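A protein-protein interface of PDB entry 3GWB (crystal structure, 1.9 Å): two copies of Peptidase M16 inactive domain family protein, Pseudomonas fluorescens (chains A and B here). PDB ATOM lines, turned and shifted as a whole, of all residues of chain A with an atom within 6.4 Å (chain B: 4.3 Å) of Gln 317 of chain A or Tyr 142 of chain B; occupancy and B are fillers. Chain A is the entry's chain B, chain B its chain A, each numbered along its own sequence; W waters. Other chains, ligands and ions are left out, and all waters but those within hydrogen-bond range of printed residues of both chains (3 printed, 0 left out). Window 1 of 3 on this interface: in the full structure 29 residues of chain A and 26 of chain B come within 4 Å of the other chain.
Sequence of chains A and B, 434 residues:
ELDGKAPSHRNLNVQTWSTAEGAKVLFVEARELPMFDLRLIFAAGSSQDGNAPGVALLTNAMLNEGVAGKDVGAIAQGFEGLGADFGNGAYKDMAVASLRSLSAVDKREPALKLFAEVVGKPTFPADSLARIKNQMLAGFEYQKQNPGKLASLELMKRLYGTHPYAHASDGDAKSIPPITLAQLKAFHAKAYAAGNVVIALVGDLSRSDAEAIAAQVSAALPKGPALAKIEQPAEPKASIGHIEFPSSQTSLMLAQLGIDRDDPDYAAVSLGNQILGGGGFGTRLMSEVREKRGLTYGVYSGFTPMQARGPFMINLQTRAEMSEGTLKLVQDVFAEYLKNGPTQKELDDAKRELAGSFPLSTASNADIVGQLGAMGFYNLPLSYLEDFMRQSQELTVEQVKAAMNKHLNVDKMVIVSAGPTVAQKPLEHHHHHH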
ATOM      1  N   GLN A 145      -7.154  -2.315 -30.488  1.00  0.00           N
ATOM      2  CA  GLN A 145      -8.298  -1.709 -29.825  1.00  0.00           C
ATOM      3  C   GLN A 145      -9.171  -2.794 -29.197  1.00  0.00           C
ATOM      4  O   GLN A 145     -10.296  -2.536 -28.757  1.00  0.00           O
ATOM      5  CB  GLN A 145      -9.091  -0.875 -30.834  1.00  0.00           C
ATOM      6  CG  GLN A 145      -8.304   0.336 -31.339  1.00  0.00           C
ATOM      7  CD  GLN A 145      -8.849   0.911 -32.635  1.00  0.00           C
ATOM      8  OE1 GLN A 145     -10.036   1.215 -32.744  1.00  0.00           O
ATOM      9  NE2 GLN A 145      -7.975   1.069 -33.627  1.00  0.00           N
ATOM     10  N   PRO A 147      -8.722  -5.458 -26.213  1.00  0.00           N
ATOM     11  CA  PRO A 147      -7.948  -5.957 -25.067  1.00  0.00           C
ATOM     12  C   PRO A 147      -7.728  -7.464 -25.080  1.00  0.00           C
ATOM     13  O   PRO A 147      -6.601  -7.942 -24.896  1.00  0.00           O
ATOM     14  CB  PRO A 147      -8.782  -5.524 -23.863  1.00  0.00           C
ATOM     15  CG  PRO A 147      -9.529  -4.330 -24.369  1.00  0.00           C
ATOM     16  CD  PRO A 147      -9.914  -4.722 -25.759  1.00  0.00           C
ATOM     17  N   GLY A 148      -8.816  -8.202 -25.286  1.00  0.00           N
ATOM     18  CA  GLY A 148      -8.756  -9.650 -25.312  1.00  0.00           C
ATOM     19  C   GLY A 148      -7.766 -10.176 -26.328  1.00  0.00           C
ATOM     20  O   GLY A 148      -6.995 -11.079 -26.032  1.00  0.00           O
ATOM     21  N   SER A 247     -10.440   1.704 -20.681  1.00  0.00           N
ATOM     22  CA  SER A 247     -11.735   1.051 -20.545  1.00  0.00           C
ATOM     23  C   SER A 247     -12.037   0.906 -19.068  1.00  0.00           C
ATOM     24  O   SER A 247     -11.138   1.002 -18.235  1.00  0.00           O
ATOM     25  CB  SER A 247     -11.701  -0.340 -21.186  1.00  0.00           C
ATOM     26  OG  SER A 247     -12.928  -1.022 -21.005  1.00  0.00           O
ATOM     27  N   GLN A 249     -13.386  -1.776 -18.143  1.00  0.00           N
ATOM     28  CA  GLN A 249     -13.285  -3.234 -18.078  1.00  0.00           C
ATOM     29  C   GLN A 249     -11.845  -3.729 -18.171  1.00  0.00           C
ATOM     30  O   GLN A 249     -10.967  -3.025 -18.671  1.00  0.00           O
ATOM     31  CB  GLN A 249     -14.092  -3.862 -19.218  1.00  0.00           C
ATOM     32  CG  GLN A 249     -15.577  -3.541 -19.189  1.00  0.00           C
ATOM     33  CD  GLN A 249     -16.332  -4.374 -18.174  1.00  0.00           C
ATOM     34  OE1 GLN A 249     -16.524  -5.582 -18.356  1.00  0.00           O
ATOM     35  NE2 GLN A 249     -16.755  -3.735 -17.089  1.00  0.00           N
ATOM     36  N   THR A 250     -11.616  -4.951 -17.690  1.00  0.00           N
ATOM     37  CA  THR A 250     -10.298  -5.574 -17.723  1.00  0.00           C
ATOM     38  C   THR A 250     -10.399  -7.029 -18.190  1.00  0.00           C
ATOM     39  O   THR A 250     -11.144  -7.829 -17.615  1.00  0.00           O
ATOM     40  CB  THR A 250      -9.617  -5.563 -16.329  1.00  0.00           C
ATOM     41  OG1 THR A 250      -9.315  -4.213 -15.943  1.00  0.00           O
ATOM     42  CG2 THR A 250      -8.322  -6.374 -16.363  1.00  0.00           C
ATOM     43  N   SER A 251      -9.654  -7.367 -19.236  1.00  0.00           N
ATOM     44  CA  SER A 251      -9.650  -8.731 -19.742  1.00  0.00           C
ATOM     45  C   SER A 251      -8.568  -9.481 -18.978  1.00  0.00           C
ATOM     46  O   SER A 251      -7.446  -8.996 -18.854  1.00  0.00           O
ATOM     47  CB  SER A 251      -9.330  -8.754 -21.239  1.00  0.00           C
ATOM     48  OG  SER A 251     -10.313  -8.058 -21.981  1.00  0.00           O
ATOM     49  N   LEU A 252      -8.916 -10.653 -18.460  1.00  0.00           N
ATOM     50  CA  LEU A 252      -7.985 -11.480 -17.706  1.00  0.00           C
ATOM     51  C   LEU A 252      -7.858 -12.844 -18.368  1.00  0.00           C
ATOM     52  O   LEU A 252      -8.861 -13.470 -18.708  1.00  0.00           O
ATOM     53  CB  LEU A 252      -8.494 -11.681 -16.280  1.00  0.00           C
ATOM     54  CG  LEU A 252      -8.670 -10.422 -15.438  1.00  0.00           C
ATOM     55  CD1 LEU A 252      -9.439 -10.764 -14.173  1.00  0.00           C
ATOM     56  CD2 LEU A 252      -7.300  -9.839 -15.110  1.00  0.00           C
ATOM     57  N   LEU A 295     -19.487 -10.841 -10.777  1.00  0.00           N
ATOM     58  CA  LEU A 295     -18.273 -10.125 -11.162  1.00  0.00           C
ATOM     59  C   LEU A 295     -17.972 -10.174 -12.668  1.00  0.00           C
ATOM     60  O   LEU A 295     -17.086  -9.473 -13.152  1.00  0.00           O
ATOM     61  CB  LEU A 295     -17.078 -10.688 -10.389  1.00  0.00           C
ATOM     62  CG  LEU A 295     -17.123 -10.565  -8.862  1.00  0.00           C
ATOM     63  CD1 LEU A 295     -16.105 -11.507  -8.253  1.00  0.00           C
ATOM     64  CD2 LEU A 295     -16.855  -9.122  -8.441  1.00  0.00           C
ATOM     65  N   THR A 296     -18.707 -10.991 -13.410  1.00  0.00           N
ATOM     66  CA  THR A 296     -18.461 -11.100 -14.846  1.00  0.00           C
ATOM     67  C   THR A 296     -19.698 -11.637 -15.553  1.00  0.00           C
ATOM     68  O   THR A 296     -20.549 -12.264 -14.925  1.00  0.00           O
ATOM     69  CB  THR A 296     -17.286 -12.066 -15.137  1.00  0.00           C
ATOM     70  OG1 THR A 296     -16.977 -12.044 -16.536  1.00  0.00           O
ATOM     71  CG2 THR A 296     -17.666 -13.493 -14.764  1.00  0.00           C
ATOM     72  N   TYR A 297     -19.804 -11.380 -16.854  1.00  0.00           N
ATOM     73  CA  TYR A 297     -20.936 -11.886 -17.626  1.00  0.00           C
ATOM     74  C   TYR A 297     -20.565 -13.259 -18.175  1.00  0.00           C
ATOM     75  O   TYR A 297     -21.413 -13.992 -18.667  1.00  0.00           O
ATOM     76  CB  TYR A 297     -21.286 -10.938 -18.779  1.00  0.00           C
ATOM     77  CG  TYR A 297     -22.059  -9.715 -18.341  1.00  0.00           C
ATOM     78  CD1 TYR A 297     -23.274  -9.846 -17.673  1.00  0.00           C
ATOM     79  CD2 TYR A 297     -21.566  -8.430 -18.566  1.00  0.00           C
ATOM     80  CE1 TYR A 297     -23.982  -8.734 -17.232  1.00  0.00           C
ATOM     81  CE2 TYR A 297     -22.270  -7.301 -18.126  1.00  0.00           C
ATOM     82  CZ  TYR A 297     -23.477  -7.466 -17.461  1.00  0.00           C
ATOM     83  OH  TYR A 297     -24.188  -6.369 -17.024  1.00  0.00           O
ATOM     84  N   GLY A 298     -19.290 -13.614 -18.075  1.00  0.00           N
ATOM     85  CA  GLY A 298     -18.876 -14.905 -18.581  1.00  0.00           C
ATOM     86  C   GLY A 298     -17.428 -15.253 -18.336  1.00  0.00           C
ATOM     87  O   GLY A 298     -16.524 -14.472 -18.642  1.00  0.00           O
ATOM     88  N   VAL A 299     -17.209 -16.434 -17.770  1.00  0.00           N
ATOM     89  CA  VAL A 299     -15.857 -16.918 -17.495  1.00  0.00           C
ATOM     90  C   VAL A 299     -15.762 -18.330 -18.047  1.00  0.00           C
ATOM     91  O   VAL A 299     -16.621 -19.172 -17.764  1.00  0.00           O
ATOM     92  CB  VAL A 299     -15.538 -16.914 -15.981  1.00  0.00           C
ATOM     93  CG1 VAL A 299     -16.636 -17.629 -15.205  1.00  0.00           C
ATOM     94  CG2 VAL A 299     -14.173 -17.568 -15.739  1.00  0.00           C
ATOM     95  N   ASN A 315     -10.342 -17.553 -19.299  1.00  0.00           N
ATOM     96  CA  ASN A 315     -10.509 -16.152 -19.659  1.00  0.00           C
ATOM     97  C   ASN A 315     -11.829 -15.569 -19.197  1.00  0.00           C
ATOM     98  O   ASN A 315     -12.843 -16.257 -19.110  1.00  0.00           O
ATOM     99  CB  ASN A 315     -10.370 -15.953 -21.172  1.00  0.00           C
ATOM    100  CG  ASN A 315     -11.355 -16.774 -21.960  1.00  0.00           C
ATOM    101  OD1 ASN A 315     -11.140 -17.965 -22.197  1.00  0.00           O
ATOM    102  ND2 ASN A 315     -12.453 -16.149 -22.365  1.00  0.00           N
ATOM    103  N   LEU A 316     -11.799 -14.281 -18.901  1.00  0.00           N
ATOM    104  CA  LEU A 316     -12.983 -13.581 -18.453  1.00  0.00           C
ATOM    105  C   LEU A 316     -12.711 -12.088 -18.399  1.00  0.00           C
ATOM    106  O   LEU A 316     -11.558 -11.645 -18.450  1.00  0.00           O
ATOM    107  CB  LEU A 316     -13.441 -14.123 -17.086  1.00  0.00           C
ATOM    108  CG  LEU A 316     -12.639 -14.077 -15.770  1.00  0.00           C
ATOM    109  CD1 LEU A 316     -11.154 -14.254 -16.017  1.00  0.00           C
ATOM    110  CD2 LEU A 316     -12.920 -12.777 -15.065  1.00  0.00           C
ATOM    111  N   GLN A 317     -13.784 -11.313 -18.322  1.00  0.00           N
ATOM    112  CA  GLN A 317     -13.683  -9.867 -18.267  1.00  0.00           C
ATOM    113  C   GLN A 317     -14.445  -9.370 -17.054  1.00  0.00           C
ATOM    114  O   GLN A 317     -15.494  -9.912 -16.711  1.00  0.00           O
ATOM    115  CB  GLN A 317     -14.270  -9.264 -19.544  1.00  0.00           C
ATOM    116  CG  GLN A 317     -14.202  -7.758 -19.629  1.00  0.00           C
ATOM    117  CD  GLN A 317     -14.509  -7.258 -21.029  1.00  0.00           C
ATOM    118  OE1 GLN A 317     -13.846  -7.645 -21.994  1.00  0.00           O
ATOM    119  NE2 GLN A 317     -15.516  -6.396 -21.149  1.00  0.00           N
ATOM    120  N   THR A 318     -13.907  -8.349 -16.393  1.00  0.00           N
ATOM    121  CA  THR A 318     -14.561  -7.777 -15.222  1.00  0.00           C
ATOM    122  C   THR A 318     -14.307  -6.281 -15.172  1.00  0.00           C
ATOM    123  O   THR A 318     -13.536  -5.750 -15.969  1.00  0.00           O
ATOM    124  CB  THR A 318     -14.024  -8.390 -13.904  1.00  0.00           C
ATOM    125  OG1 THR A 318     -12.661  -7.982 -13.706  1.00  0.00           O
ATOM    126  CG2 THR A 318     -14.089  -9.907 -13.952  1.00  0.00           C
ATOM    127  N   ARG A 319     -14.975  -5.610 -14.240  1.00  0.00           N
ATOM    128  CA  ARG A 319     -14.792  -4.177 -14.041  1.00  0.00           C
ATOM    129  C   ARG A 319     -13.352  -4.019 -13.579  1.00  0.00           C
ATOM    130  O   ARG A 319     -12.896  -4.754 -12.704  1.00  0.00           O
ATOM    131  CB  ARG A 319     -15.730  -3.669 -12.946  1.00  0.00           C
ATOM    132  CG  ARG A 319     -17.209  -3.833 -13.238  1.00  0.00           C
ATOM    133  CD  ARG A 319     -17.707  -2.839 -14.278  1.00  0.00           C
ATOM    134  NE  ARG A 319     -19.165  -2.897 -14.410  1.00  0.00           N
ATOM    135  CZ  ARG A 319     -19.881  -2.120 -15.219  1.00  0.00           C
ATOM    136  NH1 ARG A 319     -19.282  -1.214 -15.983  1.00  0.00           N
ATOM    137  NH2 ARG A 319     -21.203  -2.246 -15.259  1.00  0.00           N
ATOM    138  N   ALA B 138     -23.145  -8.047 -22.151  1.00  0.00           N
ATOM    139  CA  ALA B 138     -21.708  -8.214 -22.334  1.00  0.00           C
ATOM    140  C   ALA B 138     -21.295  -7.395 -23.553  1.00  0.00           C
ATOM    141  O   ALA B 138     -20.219  -6.785 -23.580  1.00  0.00           O
ATOM    142  CB  ALA B 138     -21.372  -9.682 -22.552  1.00  0.00           C
ATOM    143  N   GLY B 139     -22.163  -7.385 -24.560  1.00  0.00           N
ATOM    144  CA  GLY B 139     -21.890  -6.631 -25.770  1.00  0.00           C
ATOM    145  C   GLY B 139     -21.708  -5.147 -25.508  1.00  0.00           C
ATOM    146  O   GLY B 139     -20.828  -4.520 -26.094  1.00  0.00           O
ATOM    147  N   PHE B 140     -22.536  -4.574 -24.638  1.00  0.00           N
ATOM    148  CA  PHE B 140     -22.429  -3.150 -24.325  1.00  0.00           C
ATOM    149  C   PHE B 140     -21.079  -2.825 -23.699  1.00  0.00           C
ATOM    150  O   PHE B 140     -20.523  -1.751 -23.927  1.00  0.00           O
ATOM    151  CB  PHE B 140     -23.539  -2.715 -23.370  1.00  0.00           C
ATOM    152  CG  PHE B 140     -24.922  -2.860 -23.935  1.00  0.00           C
ATOM    153  CD1 PHE B 140     -25.222  -2.373 -25.206  1.00  0.00           C
ATOM    154  CD2 PHE B 140     -25.921  -3.493 -23.205  1.00  0.00           C
ATOM    155  CE1 PHE B 140     -26.500  -2.499 -25.733  1.00  0.00           C
ATOM    156  CE2 PHE B 140     -27.209  -3.624 -23.725  1.00  0.00           C
ATOM    157  CZ  PHE B 140     -27.494  -3.133 -24.996  1.00  0.00           C
ATOM    158  N   GLU B 141     -20.561  -3.754 -22.901  1.00  0.00           N
ATOM    159  CA  GLU B 141     -19.272  -3.568 -22.247  1.00  0.00           C
ATOM    160  C   GLU B 141     -18.151  -3.564 -23.279  1.00  0.00           C
ATOM    161  O   GLU B 141     -17.271  -2.706 -23.244  1.00  0.00           O
ATOM    162  CB  GLU B 141     -19.035  -4.679 -21.225  1.00  0.00           C
ATOM    163  CG  GLU B 141     -20.030  -4.670 -20.080  1.00  0.00           C
ATOM    164  CD  GLU B 141     -19.997  -3.371 -19.300  1.00  0.00           C
ATOM    165  OE1 GLU B 141     -18.982  -3.108 -18.621  1.00  0.00           O
ATOM    166  OE2 GLU B 141     -20.981  -2.604 -19.370  1.00  0.00           O
ATOM    167  N   TYR B 142     -18.187  -4.526 -24.196  1.00  0.00           N
ATOM    168  CA  TYR B 142     -17.178  -4.619 -25.244  1.00  0.00           C
ATOM    169  C   TYR B 142     -17.201  -3.359 -26.101  1.00  0.00           C
ATOM    170  O   TYR B 142     -16.154  -2.835 -26.479  1.00  0.00           O
ATOM    171  CB  TYR B 142     -17.445  -5.835 -26.136  1.00  0.00           C
ATOM    172  CG  TYR B 142     -17.217  -7.174 -25.467  1.00  0.00           C
ATOM    173  CD1 TYR B 142     -15.946  -7.554 -25.041  1.00  0.00           C
ATOM    174  CD2 TYR B 142     -18.268  -8.071 -25.283  1.00  0.00           C
ATOM    175  CE1 TYR B 142     -15.723  -8.798 -24.450  1.00  0.00           C
ATOM    176  CE2 TYR B 142     -18.062  -9.316 -24.691  1.00  0.00           C
ATOM    177  CZ  TYR B 142     -16.786  -9.674 -24.279  1.00  0.00           C
ATOM    178  OH  TYR B 142     -16.572 -10.909 -23.703  1.00  0.00           O
ATOM    179  N   GLN B 143     -18.407  -2.880 -26.392  1.00  0.00           N
ATOM    180  CA  GLN B 143     -18.612  -1.691 -27.217  1.00  0.00           C
ATOM    181  C   GLN B 143     -17.881  -0.431 -26.767  1.00  0.00           C
ATOM    182  O   GLN B 143     -17.385   0.328 -27.602  1.00  0.00           O
ATOM    183  CB  GLN B 143     -20.107  -1.374 -27.317  1.00  0.00           C
ATOM    184  CG  GLN B 143     -20.805  -1.989 -28.507  1.00  0.00           C
ATOM    185  CD  GLN B 143     -22.303  -1.764 -28.465  1.00  0.00           C
ATOM    186  OE1 GLN B 143     -22.765  -0.710 -28.028  1.00  0.00           O
ATOM    187  NE2 GLN B 143     -23.067  -2.746 -28.927  1.00  0.00           N
ATOM    188  N   LYS B 144     -17.824  -0.195 -25.462  1.00  0.00           N
ATOM    189  CA  LYS B 144     -17.158   1.002 -24.960  1.00  0.00           C
ATOM    190  C   LYS B 144     -15.636   0.943 -25.045  1.00  0.00           C
ATOM    191  O   LYS B 144     -14.949   1.900 -24.688  1.00  0.00           O
ATOM    192  CB  LYS B 144     -17.607   1.294 -23.527  1.00  0.00           C
ATOM    193  CG  LYS B 144     -17.712   0.078 -22.628  1.00  0.00           C
ATOM    194  CD  LYS B 144     -18.475   0.427 -21.358  1.00  0.00           C
ATOM    195  CE  LYS B 144     -18.603  -0.773 -20.436  1.00  0.00           C
ATOM    196  NZ  LYS B 144     -19.465  -0.481 -19.255  1.00  0.00           N
ATOM    197  N   GLN B 145     -15.116  -0.180 -25.525  1.00  0.00           N
ATOM    198  CA  GLN B 145     -13.673  -0.357 -25.679  1.00  0.00           C
ATOM    199  C   GLN B 145     -13.361  -0.171 -27.155  1.00  0.00           C
ATOM    200  O   GLN B 145     -12.230  -0.380 -27.600  1.00  0.00           O
ATOM    201  CB  GLN B 145     -13.260  -1.765 -25.242  1.00  0.00           C
ATOM    202  CG  GLN B 145     -13.746  -2.140 -23.849  1.00  0.00           C
ATOM    203  CD  GLN B 145     -13.341  -3.546 -23.441  1.00  0.00           C
ATOM    204  OE1 GLN B 145     -13.668  -4.523 -24.115  1.00  0.00           O
ATOM    205  NE2 GLN B 145     -12.626  -3.654 -22.325  1.00  0.00           N
ATOM    206  N   ASN B 146     -14.387   0.231 -27.902  1.00  0.00           N
ATOM    207  CA  ASN B 146     -14.297   0.438 -29.342  1.00  0.00           C
ATOM    208  C   ASN B 146     -14.564   1.896 -29.716  1.00  0.00           C
ATOM    209  O   ASN B 146     -15.697   2.376 -29.614  1.00  0.00           O
ATOM    210  CB  ASN B 146     -15.320  -0.462 -30.041  1.00  0.00           C
ATOM    211  CG  ASN B 146     -15.202  -0.427 -31.548  1.00  0.00           C
ATOM    212  OD1 ASN B 146     -15.073   0.640 -32.151  1.00  0.00           O
ATOM    213  ND2 ASN B 146     -15.261  -1.601 -32.172  1.00  0.00           N
HETATM  214  O   HOH W   1     -12.425  -2.180 -31.386  1.00  0.00           O
HETATM  215  O   HOH W   2     -11.389  -5.811 -21.613  1.00  0.00           O
HETATM  216  O   HOH W   3     -12.993  -3.224 -29.058  1.00  0.00           O
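Printed residues of chain B within 4 Å of Gln 145 of chain A: Gln 145 (3.1 Å).
Printed residues of chain B within 4 Å of Tyr 297 of chain A: Ala 138 and Glu 141.
Gln 317 of chain A touches just these residues of chain B: Glu 141, Tyr 142 and Gln 145.
Of chain A, only Gln 317 comes within 4 Å of Tyr 142 of chain B.
The nearest printed residue of chain B that does not touch Gln 317 of chain A is Ala 138 of chain B (5.3 Å).
The nearest printed residue of chain B that does not touch Arg 319 of chain A is Phe 140 of chain B (8.1 Å).
CG of Pro 147 of chain A touches NE2 of Gln 145 of chain B, 3.8 Å away.
CB of Gln 249 of chain A touches NE2 of Gln 145 of chain B (3.4 Å).
CD2 of Tyr 297 of chain A touches CA of Ala 138 of chain B, 3.8 Å away.
Tyr 297 of chain A touches Glu 141 of chain B (CE2 to CG, 3.97 Å).
Glu 141 of chain B touches Gln 317 of chain A (CB to NE2, 3.9 Å).
Gln 317 of chain A touches Tyr 142 of chain B (OE1 to CE1, 3.3 Å).
Gln 317 of chain A touches Gln 145 of chain B (OE1 to OE1, 3.8 Å).
The side-chain amide nitrogen (NE2) of Gln 249 of chain A sits at hydrogen-bond distance from the side-chain carboxylate (OE1) of Glu 141 of chain B, 2.8 Å away.
The side-chain carboxylate (OE1) of Glu 141 of chain B is in salt-bridge range of the guanidinium group (NH1) of Arg 319 of chain A.
The side-chain hydroxyl (OG) of Ser 247 of chain A sits at hydrogen-bond distance from the side-chain amide nitrogen (NE2) of Gln 145 of chain B, at 3.0 Å.
O of Gln 145 of chain B lies close to O of Gln 145 of chain A.
The guanidinium group (NH1) of Arg 319 of chain A lies close to the side-chain amino group (NZ) of Lys 144 of chain B (3.4 Å).
The side-chain amino group (NZ) of Lys 144 of chain B is in salt-bridge range of the side-chain carboxylate (OE2) of Glu 141 of chain B (2.6 Å).
The side-chain hydroxyl (OG) of Ser 247 of chain A lies within hydrogen-bond range of the backbone NH (N) of Gln 249 of chain A, at 3.0 Å.
The side-chain amide oxygen (OE1) of Gln 249 of chain A is in hydrogen-bond range of the side-chain amide nitrogen (NE2) of Gln 317 of chain A.
The side-chain hydroxyl of Thr 296 of chain A lies within hydrogen-bond range of the backbone carbonyl oxygen of Gln 317 of chain A (2.6 Å).
Of the 9 printed residues of chain B, 5 touch a printed residue of chain A.
Hydrophobic or aromatic side chains of chain B within 4 Å of the printed part of chain A: Ala 138 and Tyr 142.
Hydrophobic or aromatic side chains of chain A within 4 Å of the printed part of chain B: Pro 147 and Tyr 297.
Among the printed residues, Asp or Glu carboxylates within 4 Å of a Lys or Arg side-chain nitrogen of the other chain: Arg 319 of chain A with Glu 141 of chain B.
Gln 145 of chain A touches its own counterpart, Gln 145 of chain B.
Position printed for both chains: 145.
Water W2 lies within hydrogen-bond range of the side-chain hydroxyl (OG) of Ser 251 of chain A (2.5 Å), the side-chain amide nitrogen (NE2) of Gln 145 of chain B (2.6 Å) and the side-chain amide oxygen (OE1) of Gln 317 of chain A (3.1 Å).
Water W3 lies within hydrogen-bond range of the backbone carbonyl oxygen (O) of Gln 145 of chain A and the backbone carbonyl oxygen (O) of Gln 145 of chain B.
Water W1 lies within hydrogen-bond range of the side-chain amide nitrogen (ND2) of Asn 146 of chain B and the backbone carbonyl oxygen (O) of Gln 145 of chain A.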
